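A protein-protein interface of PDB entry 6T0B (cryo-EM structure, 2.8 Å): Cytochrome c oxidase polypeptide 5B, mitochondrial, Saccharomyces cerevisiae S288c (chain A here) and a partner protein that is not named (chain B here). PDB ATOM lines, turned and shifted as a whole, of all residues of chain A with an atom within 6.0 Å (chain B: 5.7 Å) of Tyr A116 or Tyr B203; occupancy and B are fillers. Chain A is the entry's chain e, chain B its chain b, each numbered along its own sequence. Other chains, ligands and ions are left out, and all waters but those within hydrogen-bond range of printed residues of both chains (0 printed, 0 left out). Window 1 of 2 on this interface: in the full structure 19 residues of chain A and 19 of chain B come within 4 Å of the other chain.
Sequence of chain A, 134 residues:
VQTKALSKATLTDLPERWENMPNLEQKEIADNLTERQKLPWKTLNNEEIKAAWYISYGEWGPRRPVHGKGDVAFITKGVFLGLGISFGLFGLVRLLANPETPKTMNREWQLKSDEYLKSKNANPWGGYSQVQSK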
ATOM      1  N   LEU A 111      24.254   3.822  12.029  1.00  0.00           N
ATOM      2  CA  LEU A 111      23.883   4.089  13.411  1.00  0.00           C
ATOM      3  C   LEU A 111      24.799   5.133  14.031  1.00  0.00           C
ATOM      4  O   LEU A 111      24.343   6.004  14.779  1.00  0.00           O
ATOM      5  CB  LEU A 111      23.925   2.805  14.222  1.00  0.00           C
ATOM      6  CG  LEU A 111      22.879   1.778  13.839  1.00  0.00           C
ATOM      7  CD1 LEU A 111      23.296   0.454  14.353  1.00  0.00           C
ATOM      8  CD2 LEU A 111      21.579   2.157  14.447  1.00  0.00           C
ATOM      9  N   LYS A 112      26.090   5.089  13.698  1.00  0.00           N
ATOM     10  CA  LYS A 112      27.014   6.076  14.236  1.00  0.00           C
ATOM     11  C   LYS A 112      26.881   7.433  13.570  1.00  0.00           C
ATOM     12  O   LYS A 112      27.415   8.412  14.094  1.00  0.00           O
ATOM     13  CB  LYS A 112      28.439   5.578  14.106  1.00  0.00           C
ATOM     14  CG  LYS A 112      28.749   4.461  15.049  1.00  0.00           C
ATOM     15  CD  LYS A 112      29.297   4.965  16.361  1.00  0.00           C
ATOM     16  CE  LYS A 112      29.768   3.802  17.219  1.00  0.00           C
ATOM     17  NZ  LYS A 112      30.267   4.243  18.549  1.00  0.00           N
ATOM     18  N   SER A 113      26.208   7.517  12.426  1.00  0.00           N
ATOM     19  CA  SER A 113      25.858   8.817  11.869  1.00  0.00           C
ATOM     20  C   SER A 113      24.558   9.350  12.445  1.00  0.00           C
ATOM     21  O   SER A 113      24.421  10.560  12.651  1.00  0.00           O
ATOM     22  CB  SER A 113      25.764   8.742  10.352  1.00  0.00           C
ATOM     23  OG  SER A 113      24.668   7.959   9.949  1.00  0.00           O
ATOM     24  N   ASP A 114      23.606   8.465  12.735  1.00  0.00           N
ATOM     25  CA  ASP A 114      22.395   8.892  13.413  1.00  0.00           C
ATOM     26  C   ASP A 114      22.661   9.311  14.838  1.00  0.00           C
ATOM     27  O   ASP A 114      21.879  10.090  15.384  1.00  0.00           O
ATOM     28  CB  ASP A 114      21.369   7.770  13.432  1.00  0.00           C
ATOM     29  CG  ASP A 114      20.950   7.347  12.075  1.00  0.00           C
ATOM     30  OD1 ASP A 114      21.369   7.996  11.109  1.00  0.00           O
ATOM     31  OD2 ASP A 114      20.230   6.335  11.972  1.00  0.00           O
ATOM     32  N   GLU A 115      23.735   8.801  15.433  1.00  0.00           N
ATOM     33  CA  GLU A 115      24.260   9.316  16.687  1.00  0.00           C
ATOM     34  C   GLU A 115      24.512  10.814  16.605  1.00  0.00           C
ATOM     35  O   GLU A 115      23.997  11.603  17.411  1.00  0.00           O
ATOM     36  CB  GLU A 115      25.553   8.570  16.995  1.00  0.00           C
ATOM     37  CG  GLU A 115      26.229   8.965  18.270  1.00  0.00           C
ATOM     38  CD  GLU A 115      25.438   8.565  19.496  1.00  0.00           C
ATOM     39  OE1 GLU A 115      24.687   7.569  19.430  1.00  0.00           O
ATOM     40  OE2 GLU A 115      25.565   9.254  20.532  1.00  0.00           O
ATOM     41  N   TYR A 116      25.291  11.213  15.600  1.00  0.00           N
ATOM     42  CA  TYR A 116      25.630  12.612  15.374  1.00  0.00           C
ATOM     43  C   TYR A 116      24.394  13.444  15.064  1.00  0.00           C
ATOM     44  O   TYR A 116      24.238  14.556  15.582  1.00  0.00           O
ATOM     45  CB  TYR A 116      26.647  12.680  14.236  1.00  0.00           C
ATOM     46  CG  TYR A 116      27.029  14.058  13.787  1.00  0.00           C
ATOM     47  CD1 TYR A 116      27.942  14.806  14.500  1.00  0.00           C
ATOM     48  CD2 TYR A 116      26.498  14.600  12.631  1.00  0.00           C
ATOM     49  CE1 TYR A 116      28.299  16.066  14.086  1.00  0.00           C
ATOM     50  CE2 TYR A 116      26.842  15.855  12.215  1.00  0.00           C
ATOM     51  CZ  TYR A 116      27.745  16.583  12.942  1.00  0.00           C
ATOM     52  OH  TYR A 116      28.098  17.840  12.519  1.00  0.00           O
ATOM     53  N   LEU A 117      23.484  12.903  14.252  1.00  0.00           N
ATOM     54  CA  LEU A 117      22.300  13.662  13.857  1.00  0.00           C
ATOM     55  C   LEU A 117      21.323  13.831  15.010  1.00  0.00           C
ATOM     56  O   LEU A 117      20.633  14.848  15.089  1.00  0.00           O
ATOM     57  CB  LEU A 117      21.614  12.990  12.680  1.00  0.00           C
ATOM     58  CG  LEU A 117      22.481  12.932  11.435  1.00  0.00           C
ATOM     59  CD1 LEU A 117      21.816  12.102  10.391  1.00  0.00           C
ATOM     60  CD2 LEU A 117      22.713  14.307  10.930  1.00  0.00           C
ATOM     61  N   LYS A 118      21.232  12.847  15.901  1.00  0.00           N
ATOM     62  CA  LYS A 118      20.427  13.023  17.097  1.00  0.00           C
ATOM     63  C   LYS A 118      21.066  14.022  18.037  1.00  0.00           C
ATOM     64  O   LYS A 118      20.358  14.778  18.707  1.00  0.00           O
ATOM     65  CB  LYS A 118      20.236  11.681  17.797  1.00  0.00           C
ATOM     66  CG  LYS A 118      19.234  11.699  18.924  1.00  0.00           C
ATOM     67  CD  LYS A 118      19.165  10.358  19.602  1.00  0.00           C
ATOM     68  CE  LYS A 118      17.967  10.276  20.503  1.00  0.00           C
ATOM     69  NZ  LYS A 118      17.906  11.454  21.397  1.00  0.00           N
ATOM     70  N   SER A 119      22.400  14.055  18.085  1.00  0.00           N
ATOM     71  CA  SER A 119      23.070  15.046  18.916  1.00  0.00           C
ATOM     72  C   SER A 119      22.898  16.452  18.373  1.00  0.00           C
ATOM     73  O   SER A 119      22.933  17.414  19.143  1.00  0.00           O
ATOM     74  CB  SER A 119      24.550  14.724  19.033  1.00  0.00           C
ATOM     75  OG  SER A 119      25.199  14.944  17.801  1.00  0.00           O
ATOM     76  N   LYS A 120      22.701  16.598  17.068  1.00  0.00           N
ATOM     77  CA  LYS A 120      22.563  17.913  16.460  1.00  0.00           C
ATOM     78  C   LYS A 120      21.125  18.288  16.140  1.00  0.00           C
ATOM     79  O   LYS A 120      20.914  19.244  15.393  1.00  0.00           O
ATOM     80  CB  LYS A 120      23.398  17.994  15.188  1.00  0.00           C
ATOM     81  CG  LYS A 120      24.874  17.904  15.429  1.00  0.00           C
ATOM     82  CD  LYS A 120      25.326  19.008  16.334  1.00  0.00           C
ATOM     83  CE  LYS A 120      26.823  19.019  16.442  1.00  0.00           C
ATOM     84  NZ  LYS A 120      27.447  19.153  15.109  1.00  0.00           N
ATOM     85  N   ASN A 121      20.142  17.547  16.666  1.00  0.00           N
ATOM     86  CA  ASN A 121      18.701  17.805  16.508  1.00  0.00           C
ATOM     87  C   ASN A 121      18.245  17.830  15.054  1.00  0.00           C
ATOM     88  O   ASN A 121      17.360  18.603  14.701  1.00  0.00           O
ATOM     89  CB  ASN A 121      18.271  19.105  17.191  1.00  0.00           C
ATOM     90  CG  ASN A 121      18.654  19.147  18.638  1.00  0.00           C
ATOM     91  OD1 ASN A 121      19.524  19.915  19.036  1.00  0.00           O
ATOM     92  ND2 ASN A 121      18.006  18.321  19.441  1.00  0.00           N
ATOM     93  N   ASP B   1      17.331  18.885   7.129  1.00  0.00           N
ATOM     94  CA  ASP B   1      18.682  19.225   7.527  1.00  0.00           C
ATOM     95  C   ASP B   1      19.677  18.323   6.838  1.00  0.00           C
ATOM     96  O   ASP B   1      20.814  18.703   6.608  1.00  0.00           O
ATOM     97  CB  ASP B   1      18.817  19.127   9.033  1.00  0.00           C
ATOM     98  CG  ASP B   1      17.719  19.861   9.748  1.00  0.00           C
ATOM     99  OD1 ASP B   1      16.999  20.623   9.075  1.00  0.00           O
ATOM    100  OD2 ASP B   1      17.568  19.698  10.974  1.00  0.00           O
ATOM    101  N   VAL B   2      19.226  17.127   6.487  1.00  0.00           N
ATOM    102  CA  VAL B   2      20.062  16.143   5.814  1.00  0.00           C
ATOM    103  C   VAL B   2      19.131  15.232   5.022  1.00  0.00           C
ATOM    104  O   VAL B   2      17.989  15.006   5.442  1.00  0.00           O
ATOM    105  CB  VAL B   2      20.944  15.394   6.833  1.00  0.00           C
ATOM    106  CG1 VAL B   2      20.122  14.572   7.802  1.00  0.00           C
ATOM    107  CG2 VAL B   2      21.966  14.541   6.160  1.00  0.00           C
ATOM    108  N   PRO B   3      19.519  14.768   3.842  1.00  0.00           N
ATOM    109  CA  PRO B   3      18.696  13.787   3.144  1.00  0.00           C
ATOM    110  C   PRO B   3      18.674  12.457   3.862  1.00  0.00           C
ATOM    111  O   PRO B   3      19.650  12.040   4.484  1.00  0.00           O
ATOM    112  CB  PRO B   3      19.376  13.663   1.783  1.00  0.00           C
ATOM    113  CG  PRO B   3      20.702  14.228   1.976  1.00  0.00           C
ATOM    114  CD  PRO B   3      20.528  15.321   2.940  1.00  0.00           C
ATOM    115  N   GLN B  11      13.328  18.334   2.595  1.00  0.00           N
ATOM    116  CA  GLN B  11      13.970  18.322   3.892  1.00  0.00           C
ATOM    117  C   GLN B  11      13.231  19.261   4.834  1.00  0.00           C
ATOM    118  O   GLN B  11      12.486  20.147   4.410  1.00  0.00           O
ATOM    119  CB  GLN B  11      15.433  18.725   3.768  1.00  0.00           C
ATOM    120  CG  GLN B  11      16.240  17.757   2.982  1.00  0.00           C
ATOM    121  CD  GLN B  11      17.636  18.228   2.766  1.00  0.00           C
ATOM    122  OE1 GLN B  11      18.241  18.819   3.646  1.00  0.00           O
ATOM    123  NE2 GLN B  11      18.164  17.977   1.584  1.00  0.00           N
ATOM    124  N   GLY B 141      31.478   7.196  11.415  1.00  0.00           N
ATOM    125  CA  GLY B 141      30.255   7.896  11.704  1.00  0.00           C
ATOM    126  C   GLY B 141      30.007   9.113  10.843  1.00  0.00           C
ATOM    127  O   GLY B 141      28.918   9.687  10.916  1.00  0.00           O
ATOM    128  N   LEU B 143      29.398  11.513   7.495  1.00  0.00           N
ATOM    129  CA  LEU B 143      28.491  11.396   6.367  1.00  0.00           C
ATOM    130  C   LEU B 143      29.273  11.615   5.087  1.00  0.00           C
ATOM    131  O   LEU B 143      29.856  12.681   4.890  1.00  0.00           O
ATOM    132  CB  LEU B 143      27.365  12.411   6.478  1.00  0.00           C
ATOM    133  CG  LEU B 143      26.287  12.150   7.520  1.00  0.00           C
ATOM    134  CD1 LEU B 143      26.638  12.730   8.877  1.00  0.00           C
ATOM    135  CD2 LEU B 143      25.012  12.733   7.052  1.00  0.00           C
ATOM    136  N   LEU B 146      29.241  14.707   2.256  1.00  0.00           N
ATOM    137  CA  LEU B 146      28.517  15.797   2.873  1.00  0.00           C
ATOM    138  C   LEU B 146      29.337  16.504   3.926  1.00  0.00           C
ATOM    139  O   LEU B 146      29.220  17.719   4.072  1.00  0.00           O
ATOM    140  CB  LEU B 146      27.239  15.290   3.491  1.00  0.00           C
ATOM    141  CG  LEU B 146      26.097  15.076   2.520  1.00  0.00           C
ATOM    142  CD1 LEU B 146      24.978  14.364   3.229  1.00  0.00           C
ATOM    143  CD2 LEU B 146      25.629  16.400   1.965  1.00  0.00           C
ATOM    144  N   ASP B 147      30.163  15.780   4.662  1.00  0.00           N
ATOM    145  CA  ASP B 147      30.907  16.387   5.746  1.00  0.00           C
ATOM    146  C   ASP B 147      32.148  17.077   5.219  1.00  0.00           C
ATOM    147  O   ASP B 147      32.721  16.686   4.205  1.00  0.00           O
ATOM    148  CB  ASP B 147      31.290  15.348   6.787  1.00  0.00           C
ATOM    149  CG  ASP B 147      30.207  15.133   7.807  1.00  0.00           C
ATOM    150  OD1 ASP B 147      29.560  16.117   8.204  1.00  0.00           O
ATOM    151  OD2 ASP B 147      29.992  13.973   8.205  1.00  0.00           O
ATOM    152  N   THR B 148      32.546  18.127   5.918  1.00  0.00           N
ATOM    153  CA  THR B 148      33.686  18.939   5.561  1.00  0.00           C
ATOM    154  C   THR B 148      34.650  18.992   6.730  1.00  0.00           C
ATOM    155  O   THR B 148      34.353  18.517   7.825  1.00  0.00           O
ATOM    156  CB  THR B 148      33.252  20.350   5.181  1.00  0.00           C
ATOM    157  OG1 THR B 148      32.441  20.889   6.226  1.00  0.00           O
ATOM    158  CG2 THR B 148      32.464  20.336   3.907  1.00  0.00           C
ATOM    159  N   ALA B 174      23.997  26.514  -2.477  1.00  0.00           N
ATOM    160  CA  ALA B 174      22.661  25.954  -2.357  1.00  0.00           C
ATOM    161  C   ALA B 174      22.562  25.157  -1.076  1.00  0.00           C
ATOM    162  O   ALA B 174      23.363  24.248  -0.847  1.00  0.00           O
ATOM    163  CB  ALA B 174      22.328  25.070  -3.551  1.00  0.00           C
ATOM    164  N   ILE B 175      21.593  25.508  -0.234  1.00  0.00           N
ATOM    165  CA  ILE B 175      21.210  24.697   0.907  1.00  0.00           C
ATOM    166  C   ILE B 175      19.696  24.553   0.871  1.00  0.00           C
ATOM    167  O   ILE B 175      18.978  25.557   0.955  1.00  0.00           O
ATOM    168  CB  ILE B 175      21.657  25.289   2.253  1.00  0.00           C
ATOM    169  CG1 ILE B 175      23.170  25.389   2.323  1.00  0.00           C
ATOM    170  CG2 ILE B 175      21.237  24.380   3.354  1.00  0.00           C
ATOM    171  CD1 ILE B 175      23.689  26.762   2.109  1.00  0.00           C
ATOM    172  N   PRO B 176      19.162  23.344   0.728  1.00  0.00           N
ATOM    173  CA  PRO B 176      17.724  23.186   0.507  1.00  0.00           C
ATOM    174  C   PRO B 176      16.862  23.364   1.742  1.00  0.00           C
ATOM    175  O   PRO B 176      15.764  23.909   1.641  1.00  0.00           O
ATOM    176  CB  PRO B 176      17.619  21.759  -0.037  1.00  0.00           C
ATOM    177  CG  PRO B 176      18.816  21.091   0.420  1.00  0.00           C
ATOM    178  CD  PRO B 176      19.888  22.100   0.452  1.00  0.00           C
ATOM    179  N   SER B 177      17.321  22.915   2.901  1.00  0.00           N
ATOM    180  CA  SER B 177      16.488  23.056   4.084  1.00  0.00           C
ATOM    181  C   SER B 177      16.452  24.492   4.568  1.00  0.00           C
ATOM    182  O   SER B 177      15.485  24.904   5.214  1.00  0.00           O
ATOM    183  CB  SER B 177      16.974  22.126   5.186  1.00  0.00           C
ATOM    184  OG  SER B 177      18.226  22.538   5.681  1.00  0.00           O
ATOM    185  N   VAL B 201      22.374  21.518  12.243  1.00  0.00           N
ATOM    186  CA  VAL B 201      23.341  21.541  11.159  1.00  0.00           C
ATOM    187  C   VAL B 201      22.619  21.164   9.875  1.00  0.00           C
ATOM    188  O   VAL B 201      21.790  20.253   9.854  1.00  0.00           O
ATOM    189  CB  VAL B 201      24.559  20.633  11.460  1.00  0.00           C
ATOM    190  CG1 VAL B 201      24.168  19.194  11.703  1.00  0.00           C
ATOM    191  CG2 VAL B 201      25.606  20.729  10.372  1.00  0.00           C
ATOM    192  N   PHE B 202      22.893  21.911   8.817  1.00  0.00           N
ATOM    193  CA  PHE B 202      22.179  21.806   7.561  1.00  0.00           C
ATOM    194  C   PHE B 202      23.199  21.656   6.457  1.00  0.00           C
ATOM    195  O   PHE B 202      24.180  22.401   6.412  1.00  0.00           O
ATOM    196  CB  PHE B 202      21.310  23.034   7.317  1.00  0.00           C
ATOM    197  CG  PHE B 202      20.654  23.561   8.553  1.00  0.00           C
ATOM    198  CD1 PHE B 202      19.485  23.008   9.017  1.00  0.00           C
ATOM    199  CD2 PHE B 202      21.205  24.605   9.250  1.00  0.00           C
ATOM    200  CE1 PHE B 202      18.893  23.484  10.152  1.00  0.00           C
ATOM    201  CE2 PHE B 202      20.611  25.073  10.376  1.00  0.00           C
ATOM    202  CZ  PHE B 202      19.456  24.519  10.823  1.00  0.00           C
ATOM    203  N   TYR B 203      22.985  20.689   5.583  1.00  0.00           N
ATOM    204  CA  TYR B 203      23.930  20.383   4.528  1.00  0.00           C
ATOM    205  C   TYR B 203      23.403  20.869   3.192  1.00  0.00           C
ATOM    206  O   TYR B 203      22.199  21.010   2.996  1.00  0.00           O
ATOM    207  CB  TYR B 203      24.202  18.888   4.443  1.00  0.00           C
ATOM    208  CG  TYR B 203      25.045  18.358   5.560  1.00  0.00           C
ATOM    209  CD1 TYR B 203      26.419  18.420   5.500  1.00  0.00           C
ATOM    210  CD2 TYR B 203      24.463  17.787   6.672  1.00  0.00           C
ATOM    211  CE1 TYR B 203      27.186  17.931   6.515  1.00  0.00           C
ATOM    212  CE2 TYR B 203      25.226  17.300   7.694  1.00  0.00           C
ATOM    213  CZ  TYR B 203      26.586  17.374   7.607  1.00  0.00           C
ATOM    214  OH  TYR B 203      27.360  16.884   8.625  1.00  0.00           O
ATOM    215  N   GLY B 204      24.327  21.113   2.276  1.00  0.00           N
ATOM    216  CA  GLY B 204      23.991  21.512   0.927  1.00  0.00           C
ATOM    217  C   GLY B 204      25.136  21.147   0.015  1.00  0.00           C
ATOM    218  O   GLY B 204      26.135  20.569   0.444  1.00  0.00           O
ATOM    219  N   ALA B 205      24.997  21.505  -1.255  1.00  0.00           N
ATOM    220  CA  ALA B 205      26.011  21.142  -2.229  1.00  0.00           C
ATOM    221  C   ALA B 205      26.035  22.150  -3.362  1.00  0.00           C
ATOM    222  O   ALA B 205      25.105  22.937  -3.536  1.00  0.00           O
ATOM    223  CB  ALA B 205      25.771  19.740  -2.776  1.00  0.00           C
ATOM    224  N   ILE B 219      28.518  21.977   1.356  1.00  0.00           N
ATOM    225  CA  ILE B 219      28.288  23.102   2.252  1.00  0.00           C
ATOM    226  C   ILE B 219      27.748  22.542   3.554  1.00  0.00           C
ATOM    227  O   ILE B 219      26.865  21.684   3.534  1.00  0.00           O
ATOM    228  CB  ILE B 219      27.290  24.104   1.652  1.00  0.00           C
ATOM    229  CG1 ILE B 219      27.625  24.426   0.206  1.00  0.00           C
ATOM    230  CG2 ILE B 219      27.242  25.371   2.452  1.00  0.00           C
ATOM    231  CD1 ILE B 219      26.562  25.198  -0.478  1.00  0.00           C
ATOM    232  N   LYS B 220      28.254  23.032   4.678  1.00  0.00           N
ATOM    233  CA  LYS B 220      27.819  22.587   5.996  1.00  0.00           C
ATOM    234  C   LYS B 220      27.633  23.802   6.889  1.00  0.00           C
ATOM    235  O   LYS B 220      28.592  24.542   7.132  1.00  0.00           O
ATOM    236  CB  LYS B 220      28.841  21.632   6.601  1.00  0.00           C
ATOM    237  CG  LYS B 220      28.494  21.152   7.974  1.00  0.00           C
ATOM    238  CD  LYS B 220      29.583  20.275   8.529  1.00  0.00           C
ATOM    239  CE  LYS B 220      29.151  19.631   9.816  1.00  0.00           C
ATOM    240  NZ  LYS B 220      30.216  18.774  10.373  1.00  0.00           N
ATOM    241  N   ILE B 221      26.414  24.003   7.387  1.00  0.00           N
ATOM    242  CA  ILE B 221      26.089  25.167   8.201  1.00  0.00           C
ATOM    243  C   ILE B 221      25.613  24.708   9.564  1.00  0.00           C
ATOM    244  O   ILE B 221      24.579  24.049   9.674  1.00  0.00           O
ATOM    245  CB  ILE B 221      25.022  26.040   7.545  1.00  0.00           C
ATOM    246  CG1 ILE B 221      25.526  26.572   6.217  1.00  0.00           C
ATOM    247  CG2 ILE B 221      24.659  27.160   8.475  1.00  0.00           C
ATOM    248  CD1 ILE B 221      24.631  27.597   5.604  1.00  0.00           C
ATOM    249  N   GLU B 222      26.356  25.072  10.594  1.00  0.00           N
ATOM    250  CA  GLU B 222      25.966  24.853  11.978  1.00  0.00           C
ATOM    251  C   GLU B 222      25.306  26.120  12.496  1.00  0.00           C
ATOM    252  O   GLU B 222      25.955  27.159  12.615  1.00  0.00           O
ATOM    253  CB  GLU B 222      27.179  24.502  12.829  1.00  0.00           C
ATOM    254  CG  GLU B 222      27.871  23.228  12.438  1.00  0.00           C
ATOM    255  CD  GLU B 222      29.093  22.956  13.292  1.00  0.00           C
ATOM    256  OE1 GLU B 222      29.366  23.759  14.209  1.00  0.00           O
ATOM    257  OE2 GLU B 222      29.788  21.946  13.049  1.00  0.00           O
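The side-chain amino group (NZ) of Lys B220 lies within hydrogen-bond range of the side-chain hydroxyl (OH) of Tyr A116, at 3.2 Å.
Printed residues of chain A that touch a printed residue of chain B: Lys A112, Ser A113, Tyr A116, Leu A117, Lys A120 and Asn A121. Hydrophobic or aromatic side chains of chain A that line the printed part of chain B: Tyr A116 and Leu A117. Hydrophobic or aromatic side chains of chain B that line the printed part of chain A: Val B2, Val B201 and Tyr B203. Among the printed residues, 7 pairs touch across the chains. Among the printed residues, no Asp or Glu carboxylate lies within 4 Å of a Lys or Arg side-chain nitrogen of the other chain.
Glu A115 touches none of the printed residues of chain B. Tyr A116 touches just these residues of chain B: Tyr B203 and Lys B220. Printed residues of chain B within 4 Å of Leu A117: Val B2 (3.96 Å). Of the printed residues of chain A, Asp B1 touches Asn A121. Asp B147 touches none of the printed residues of chain A. Of the printed residues of chain A, Val B201 touches Lys A120 (3.8 Å). Of chain A, only Tyr A116 comes within 4 Å of Tyr B203.
Among the printed residues, pairs that only touch across the chains: Lys A112 with Gly B141 (3.7 Å), Ser A113 with Gly B141 (3.3 Å), Tyr A116 with Tyr B203 (3.8 Å), Leu A117 with Val B2 (3.96 Å), Lys A120 with Val B201 (3.8 Å) and Asn A121 with Asp B1 (3.9 Å).
N of Tyr B203 sits at hydrogen-bond distance from O of Asp B1, 3.1 Å away. OE1 of Gln B11 is in hydrogen-bond range of N of Val B2. The side-chain carboxylate (OD1) of Asp B147 lies within salt-bridge range of the side-chain amino group (NZ) of Lys B220. The side-chain hydroxyl of Ser A113 is in hydrogen-bond range of the side-chain carboxylate of Asp A114. The backbone carbonyl oxygen (O) of Tyr A116 lies within hydrogen-bond range of the side-chain hydroxyl (OG) of Ser A119, at 2.4 Å. The side-chain hydroxyl (OH) of Tyr A116 sits at hydrogen-bond distance from the side-chain amino group (NZ) of Lys A120, at 3.0 Å.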
